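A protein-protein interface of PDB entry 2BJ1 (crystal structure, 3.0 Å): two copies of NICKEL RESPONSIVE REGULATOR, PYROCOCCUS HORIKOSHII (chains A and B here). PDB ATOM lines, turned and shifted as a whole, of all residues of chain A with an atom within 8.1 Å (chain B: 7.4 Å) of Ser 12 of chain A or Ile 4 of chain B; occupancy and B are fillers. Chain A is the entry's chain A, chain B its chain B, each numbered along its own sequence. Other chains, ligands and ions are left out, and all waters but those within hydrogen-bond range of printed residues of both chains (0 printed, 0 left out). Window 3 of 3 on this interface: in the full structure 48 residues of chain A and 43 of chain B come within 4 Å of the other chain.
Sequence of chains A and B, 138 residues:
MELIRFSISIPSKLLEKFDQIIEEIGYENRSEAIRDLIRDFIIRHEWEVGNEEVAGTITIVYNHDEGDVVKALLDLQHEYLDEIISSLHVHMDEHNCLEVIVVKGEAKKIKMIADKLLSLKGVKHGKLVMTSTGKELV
OG of Ser 7 of chain A sits at hydrogen-bond distance from NH1 of Arg 5 of chain B (3.3 Å).
The backbone carbonyl oxygen (O) of Phe 6 of chain B lies within hydrogen-bond range of the backbone NH (N) of Ile 8 of chain A (3.0 Å).
The side-chain hydroxyl (OG) of Ser 12 of chain A is in hydrogen-bond range of the backbone carbonyl oxygen (O) of Glu 2 of chain B, 3.1 Å away.
O of Ile 10 of chain A is in hydrogen-bond range of N of Ile 4 of chain B, at 3.0 Å.
O of Leu 15 of chain A lies close to OD1 of Asp 19 of chain A (2.7 Å).
NE of Arg 30 of chain A lies within salt-bridge range of OD2 of Asp 19 of chain A (2.8 Å).
Among the printed residues, pairs that only touch across the chains: Ser 7 of chain A with Phe 6 of chain B (2.9 Å), Ser 12 of chain A with Ile 4 of chain B (3.1 Å), Leu 15 of chain A with Ile 4 of chain B (3.2 Å), Ile 8 of chain A with Arg 5 of chain B (3.2 Å), Ile 10 of chain A with Phe 6 of chain B (3.3 Å), Ser 9 of chain A with Arg 5 of chain B (3.3 Å), Arg 30 of chain A with Phe 6 of chain B (3.4 Å), Ser 9 of chain A with Leu 3 of chain B (3.7 Å), Leu 15 of chain A with Phe 6 of chain B (3.7 Å), Ile 10 of chain A with Leu 3 of chain B (3.8 Å) and Pro 11 of chain A with Leu 3 of chain B (3.9 Å).
Of chain B, only Glu 2 and Ile 4 come within 4 Å of Ser 12 of chain A.
Of the printed residues of chain A, Ile 4 of chain B touches Ile 10, Ser 12 and Leu 15.
Of the printed residues of chain A, Leu 3 of chain B touches Ser 9 (3.7 Å), Ile 10 (3.8 Å) and Pro 11 (3.9 Å).
Printed residues of chain B within 4 Å of Pro 11 of chain A: Leu 3 (3.9 Å).
Printed residues of chain B within 4 Å of Ile 10 of chain A: Leu 3 (3.8 Å), Ile 4 (3.0 Å) and Phe 6 (3.3 Å).
Leu 14 of chain A touches none of the printed residues of chain B.
The nearest residue of chain B that does not touch Ser 12 of chain A is Leu 3 of chain B (4.7 Å).
The nearest printed residue of chain A that does not touch Ile 4 of chain B is Ile 8 of chain A (4.01 Å).
Of the 14 printed residues of chain A, 8 touch a printed residue of chain B.
Hydrophobic or aromatic side chains of chain A within 4 Å of the printed part of chain B: Ile 8, Ile 10, Pro 11 and Leu 15.
Printed residues of chain B that touch a printed residue of chain A: Glu 2, Leu 3, Ile 4, Arg 5 and Phe 6.
Hydrophobic or aromatic side chains of chain B that line the printed part of chain A: Leu 3, Ile 4 and Phe 6.
Along chain B the printed residues that touch a printed residue of chain A span positions 2 to 6.
Among the printed residues, 15 pairs touch across the chains.
Among the printed residues, no Asp or Glu carboxylate lies within 4 Å of a Lys or Arg side-chain nitrogen of the other chain.
No position is printed for both chains.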
ATOM      1  N   SER A   7      21.926  -1.223  -3.822  1.00  0.00           N
ATOM      2  CA  SER A   7      21.791   0.063  -3.125  1.00  0.00           C
ATOM      3  C   SER A   7      23.120   0.772  -2.893  1.00  0.00           C
ATOM      4  O   SER A   7      24.177   0.148  -2.920  1.00  0.00           O
ATOM      5  CB  SER A   7      21.065  -0.108  -1.786  1.00  0.00           C
ATOM      6  OG  SER A   7      21.923  -0.618  -0.793  1.00  0.00           O
ATOM      7  N   ILE A   8      23.058   2.084  -2.675  1.00  0.00           N
ATOM      8  CA  ILE A   8      24.264   2.884  -2.454  1.00  0.00           C
ATOM      9  C   ILE A   8      24.183   3.841  -1.275  1.00  0.00           C
ATOM     10  O   ILE A   8      23.118   4.376  -0.961  1.00  0.00           O
ATOM     11  CB  ILE A   8      24.616   3.754  -3.679  1.00  0.00           C
ATOM     12  CG1 ILE A   8      23.405   4.603  -4.062  1.00  0.00           C
ATOM     13  CG2 ILE A   8      25.109   2.880  -4.826  1.00  0.00           C
ATOM     14  CD1 ILE A   8      23.764   5.795  -4.885  1.00  0.00           C
ATOM     15  N   SER A   9      25.328   4.064  -0.637  1.00  0.00           N
ATOM     16  CA  SER A   9      25.409   4.982   0.488  1.00  0.00           C
ATOM     17  C   SER A   9      25.661   6.368  -0.114  1.00  0.00           C
ATOM     18  O   SER A   9      26.635   6.575  -0.846  1.00  0.00           O
ATOM     19  CB  SER A   9      26.562   4.570   1.410  1.00  0.00           C
ATOM     20  OG  SER A   9      26.476   5.198   2.674  1.00  0.00           O
ATOM     21  N   ILE A  10      24.775   7.312   0.175  1.00  0.00           N
ATOM     22  CA  ILE A  10      24.919   8.660  -0.361  1.00  0.00           C
ATOM     23  C   ILE A  10      24.592   9.743   0.664  1.00  0.00           C
ATOM     24  O   ILE A  10      23.591   9.655   1.374  1.00  0.00           O
ATOM     25  CB  ILE A  10      23.987   8.868  -1.574  1.00  0.00           C
ATOM     26  CG1 ILE A  10      24.060  10.320  -2.060  1.00  0.00           C
ATOM     27  CG2 ILE A  10      22.562   8.528  -1.186  1.00  0.00           C
ATOM     28  CD1 ILE A  10      23.079  10.653  -3.157  1.00  0.00           C
ATOM     29  N   PRO A  11      25.444  10.777   0.769  1.00  0.00           N
ATOM     30  CA  PRO A  11      25.187  11.863   1.720  1.00  0.00           C
ATOM     31  C   PRO A  11      23.858  12.598   1.444  1.00  0.00           C
ATOM     32  O   PRO A  11      23.521  12.927   0.299  1.00  0.00           O
ATOM     33  CB  PRO A  11      26.415  12.760   1.554  1.00  0.00           C
ATOM     34  CG  PRO A  11      26.977  12.386   0.216  1.00  0.00           C
ATOM     35  CD  PRO A  11      26.787  10.908   0.184  1.00  0.00           C
ATOM     36  N   SER A  12      23.114  12.850   2.515  1.00  0.00           N
ATOM     37  CA  SER A  12      21.813  13.503   2.451  1.00  0.00           C
ATOM     38  C   SER A  12      21.687  14.814   1.708  1.00  0.00           C
ATOM     39  O   SER A  12      20.929  14.899   0.758  1.00  0.00           O
ATOM     40  CB  SER A  12      21.270  13.679   3.851  1.00  0.00           C
ATOM     41  OG  SER A  12      20.888  12.418   4.350  1.00  0.00           O
ATOM     42  N   LYS A  13      22.387  15.854   2.143  1.00  0.00           N
ATOM     43  CA  LYS A  13      22.292  17.130   1.433  1.00  0.00           C
ATOM     44  C   LYS A  13      22.436  16.900  -0.080  1.00  0.00           C
ATOM     45  O   LYS A  13      21.769  17.560  -0.886  1.00  0.00           O
ATOM     46  CB  LYS A  13      23.381  18.109   1.903  1.00  0.00           C
ATOM     47  CG  LYS A  13      23.356  19.458   1.155  1.00  0.00           C
ATOM     48  CD  LYS A  13      24.756  19.924   0.732  1.00  0.00           C
ATOM     49  CE  LYS A  13      25.364  19.012  -0.334  1.00  0.00           C
ATOM     50  NZ  LYS A  13      26.750  19.408  -0.717  1.00  0.00           N
ATOM     51  N   LEU A  14      23.309  15.963  -0.450  1.00  0.00           N
ATOM     52  CA  LEU A  14      23.545  15.654  -1.843  1.00  0.00           C
ATOM     53  C   LEU A  14      22.312  15.003  -2.394  1.00  0.00           C
ATOM     54  O   LEU A  14      21.742  15.483  -3.377  1.00  0.00           O
ATOM     55  CB  LEU A  14      24.730  14.707  -2.009  1.00  0.00           C
ATOM     56  CG  LEU A  14      25.017  14.280  -3.458  1.00  0.00           C
ATOM     57  CD1 LEU A  14      25.166  15.510  -4.346  1.00  0.00           C
ATOM     58  CD2 LEU A  14      26.261  13.396  -3.513  1.00  0.00           C
ATOM     59  N   LEU A  15      21.895  13.905  -1.770  1.00  0.00           N
ATOM     60  CA  LEU A  15      20.700  13.209  -2.228  1.00  0.00           C
ATOM     61  C   LEU A  15      19.467  14.126  -2.149  1.00  0.00           C
ATOM     62  O   LEU A  15      18.439  13.841  -2.751  1.00  0.00           O
ATOM     63  CB  LEU A  15      20.463  11.945  -1.400  1.00  0.00           C
ATOM     64  CG  LEU A  15      19.257  11.107  -1.841  1.00  0.00           C
ATOM     65  CD1 LEU A  15      19.567  10.394  -3.146  1.00  0.00           C
ATOM     66  CD2 LEU A  15      18.909  10.095  -0.774  1.00  0.00           C
ATOM     67  N   GLU A  16      19.584  15.230  -1.410  1.00  0.00           N
ATOM     68  CA  GLU A  16      18.505  16.209  -1.241  1.00  0.00           C
ATOM     69  C   GLU A  16      18.316  17.072  -2.491  1.00  0.00           C
ATOM     70  O   GLU A  16      17.226  17.116  -3.056  1.00  0.00           O
ATOM     71  CB  GLU A  16      18.809  17.112  -0.037  1.00  0.00           C
ATOM     72  CG  GLU A  16      17.995  18.406   0.023  1.00  0.00           C
ATOM     73  CD  GLU A  16      16.510  18.177   0.278  1.00  0.00           C
ATOM     74  OE1 GLU A  16      16.162  17.678   1.370  1.00  0.00           O
ATOM     75  OE2 GLU A  16      15.689  18.500  -0.612  1.00  0.00           O
ATOM     76  N   LYS A  17      19.380  17.760  -2.907  1.00  0.00           N
ATOM     77  CA  LYS A  17      19.348  18.625  -4.089  1.00  0.00           C
ATOM     78  C   LYS A  17      19.047  17.827  -5.349  1.00  0.00           C
ATOM     79  O   LYS A  17      18.636  18.392  -6.362  1.00  0.00           O
ATOM     80  CB  LYS A  17      20.687  19.346  -4.274  1.00  0.00           C
ATOM     81  CG  LYS A  17      21.097  20.225  -3.104  1.00  0.00           C
ATOM     82  CD  LYS A  17      22.539  20.729  -3.245  1.00  0.00           C
ATOM     83  CE  LYS A  17      23.564  19.589  -3.170  1.00  0.00           C
ATOM     84  NZ  LYS A  17      24.973  20.055  -3.359  1.00  0.00           N
ATOM     85  N   PHE A  18      19.273  16.517  -5.289  1.00  0.00           N
ATOM     86  CA  PHE A  18      19.008  15.663  -6.436  1.00  0.00           C
ATOM     87  C   PHE A  18      17.510  15.486  -6.575  1.00  0.00           C
ATOM     88  O   PHE A  18      16.915  15.981  -7.526  1.00  0.00           O
ATOM     89  CB  PHE A  18      19.679  14.299  -6.277  1.00  0.00           C
ATOM     90  CG  PHE A  18      19.650  13.462  -7.532  1.00  0.00           C
ATOM     91  CD1 PHE A  18      19.967  14.031  -8.776  1.00  0.00           C
ATOM     92  CD2 PHE A  18      19.350  12.105  -7.474  1.00  0.00           C
ATOM     93  CE1 PHE A  18      19.990  13.257  -9.941  1.00  0.00           C
ATOM     94  CE2 PHE A  18      19.370  11.328  -8.627  1.00  0.00           C
ATOM     95  CZ  PHE A  18      19.691  11.904  -9.866  1.00  0.00           C
ATOM     96  N   ASP A  19      16.903  14.786  -5.623  1.00  0.00           N
ATOM     97  CA  ASP A  19      15.464  14.568  -5.639  1.00  0.00           C
ATOM     98  C   ASP A  19      14.764  15.890  -5.910  1.00  0.00           C
ATOM     99  O   ASP A  19      13.794  15.961  -6.666  1.00  0.00           O
ATOM    100  CB  ASP A  19      14.997  14.014  -4.291  1.00  0.00           C
ATOM    101  CG  ASP A  19      15.436  12.581  -4.064  1.00  0.00           C
ATOM    102  OD1 ASP A  19      16.654  12.345  -4.036  1.00  0.00           O
ATOM    103  OD2 ASP A  19      14.569  11.688  -3.916  1.00  0.00           O
ATOM    104  N   ARG A  30      13.768   7.933  -8.568  1.00  0.00           N
ATOM    105  CA  ARG A  30      15.196   8.241  -8.652  1.00  0.00           C
ATOM    106  C   ARG A  30      15.816   7.249  -9.606  1.00  0.00           C
ATOM    107  O   ARG A  30      16.792   7.547 -10.296  1.00  0.00           O
ATOM    108  CB  ARG A  30      15.911   8.082  -7.306  1.00  0.00           C
ATOM    109  CG  ARG A  30      15.465   8.988  -6.201  1.00  0.00           C
ATOM    110  CD  ARG A  30      16.552   9.056  -5.161  1.00  0.00           C
ATOM    111  NE  ARG A  30      16.031   9.298  -3.821  1.00  0.00           N
ATOM    112  CZ  ARG A  30      15.615   8.340  -3.008  1.00  0.00           C
ATOM    113  NH1 ARG A  30      15.657   7.072  -3.396  1.00  0.00           N
ATOM    114  NH2 ARG A  30      15.160   8.649  -1.806  1.00  0.00           N
ATOM    115  N   MET B   1      28.253  13.726   5.695  1.00  0.00           N
ATOM    116  CA  MET B   1      27.915  14.372   7.014  1.00  0.00           C
ATOM    117  C   MET B   1      26.897  13.523   7.783  1.00  0.00           C
ATOM    118  O   MET B   1      26.912  13.471   9.016  1.00  0.00           O
ATOM    119  CB  MET B   1      27.368  15.799   6.795  1.00  0.00           C
ATOM    120  CG  MET B   1      27.557  16.755   8.001  1.00  0.00           C
ATOM    121  SD  MET B   1      27.435  18.553   7.625  1.00  0.00           S
ATOM    122  CE  MET B   1      29.037  18.893   6.851  1.00  0.00           C
ATOM    123  N   GLU B   2      26.006  12.880   7.032  1.00  0.00           N
ATOM    124  CA  GLU B   2      24.989  11.973   7.562  1.00  0.00           C
ATOM    125  C   GLU B   2      24.471  11.198   6.352  1.00  0.00           C
ATOM    126  O   GLU B   2      23.570  11.641   5.641  1.00  0.00           O
ATOM    127  CB  GLU B   2      23.851  12.726   8.246  1.00  0.00           C
ATOM    128  CG  GLU B   2      23.054  11.807   9.154  1.00  0.00           C
ATOM    129  CD  GLU B   2      23.968  10.921  10.003  1.00  0.00           C
ATOM    130  OE1 GLU B   2      24.655  11.448  10.906  1.00  0.00           O
ATOM    131  OE2 GLU B   2      24.011   9.696   9.756  1.00  0.00           O
ATOM    132  N   LEU B   3      25.066  10.032   6.138  1.00  0.00           N
ATOM    133  CA  LEU B   3      24.777   9.182   4.992  1.00  0.00           C
ATOM    134  C   LEU B   3      23.482   8.380   5.010  1.00  0.00           C
ATOM    135  O   LEU B   3      23.207   7.679   5.983  1.00  0.00           O
ATOM    136  CB  LEU B   3      25.949   8.215   4.807  1.00  0.00           C
ATOM    137  CG  LEU B   3      27.370   8.762   4.973  1.00  0.00           C
ATOM    138  CD1 LEU B   3      28.348   7.684   4.584  1.00  0.00           C
ATOM    139  CD2 LEU B   3      27.594   9.981   4.095  1.00  0.00           C
ATOM    140  N   ILE B   4      22.702   8.474   3.928  1.00  0.00           N
ATOM    141  CA  ILE B   4      21.453   7.713   3.792  1.00  0.00           C
ATOM    142  C   ILE B   4      21.500   6.808   2.556  1.00  0.00           C
ATOM    143  O   ILE B   4      21.725   7.268   1.439  1.00  0.00           O
ATOM    144  CB  ILE B   4      20.186   8.623   3.708  1.00  0.00           C
ATOM    145  CG1 ILE B   4      20.229   9.517   2.471  1.00  0.00           C
ATOM    146  CG2 ILE B   4      20.070   9.456   4.974  1.00  0.00           C
ATOM    147  CD1 ILE B   4      19.042  10.470   2.371  1.00  0.00           C
ATOM    148  N   ARG B   5      21.288   5.516   2.782  1.00  0.00           N
ATOM    149  CA  ARG B   5      21.325   4.497   1.739  1.00  0.00           C
ATOM    150  C   ARG B   5      19.942   4.214   1.167  1.00  0.00           C
ATOM    151  O   ARG B   5      18.954   4.160   1.894  1.00  0.00           O
ATOM    152  CB  ARG B   5      21.931   3.224   2.329  1.00  0.00           C
ATOM    153  CG  ARG B   5      21.961   2.008   1.431  1.00  0.00           C
ATOM    154  CD  ARG B   5      22.695   0.848   2.125  1.00  0.00           C
ATOM    155  NE  ARG B   5      24.104   1.155   2.389  1.00  0.00           N
ATOM    156  CZ  ARG B   5      25.102   0.964   1.524  1.00  0.00           C
ATOM    157  NH1 ARG B   5      24.866   0.451   0.325  1.00  0.00           N
ATOM    158  NH2 ARG B   5      26.343   1.301   1.853  1.00  0.00           N
ATOM    159  N   PHE B   6      19.880   4.059  -0.151  1.00  0.00           N
ATOM    160  CA  PHE B   6      18.636   3.767  -0.860  1.00  0.00           C
ATOM    161  C   PHE B   6      19.002   2.782  -1.970  1.00  0.00           C
ATOM    162  O   PHE B   6      20.177   2.631  -2.299  1.00  0.00           O
ATOM    163  CB  PHE B   6      18.017   5.042  -1.462  1.00  0.00           C
ATOM    164  CG  PHE B   6      18.814   5.625  -2.577  1.00  0.00           C
ATOM    165  CD1 PHE B   6      19.936   6.394  -2.315  1.00  0.00           C
ATOM    166  CD2 PHE B   6      18.499   5.325  -3.890  1.00  0.00           C
ATOM    167  CE1 PHE B   6      20.736   6.845  -3.339  1.00  0.00           C
ATOM    168  CE2 PHE B   6      19.295   5.772  -4.928  1.00  0.00           C
ATOM    169  CZ  PHE B   6      20.419   6.532  -4.651  1.00  0.00           C
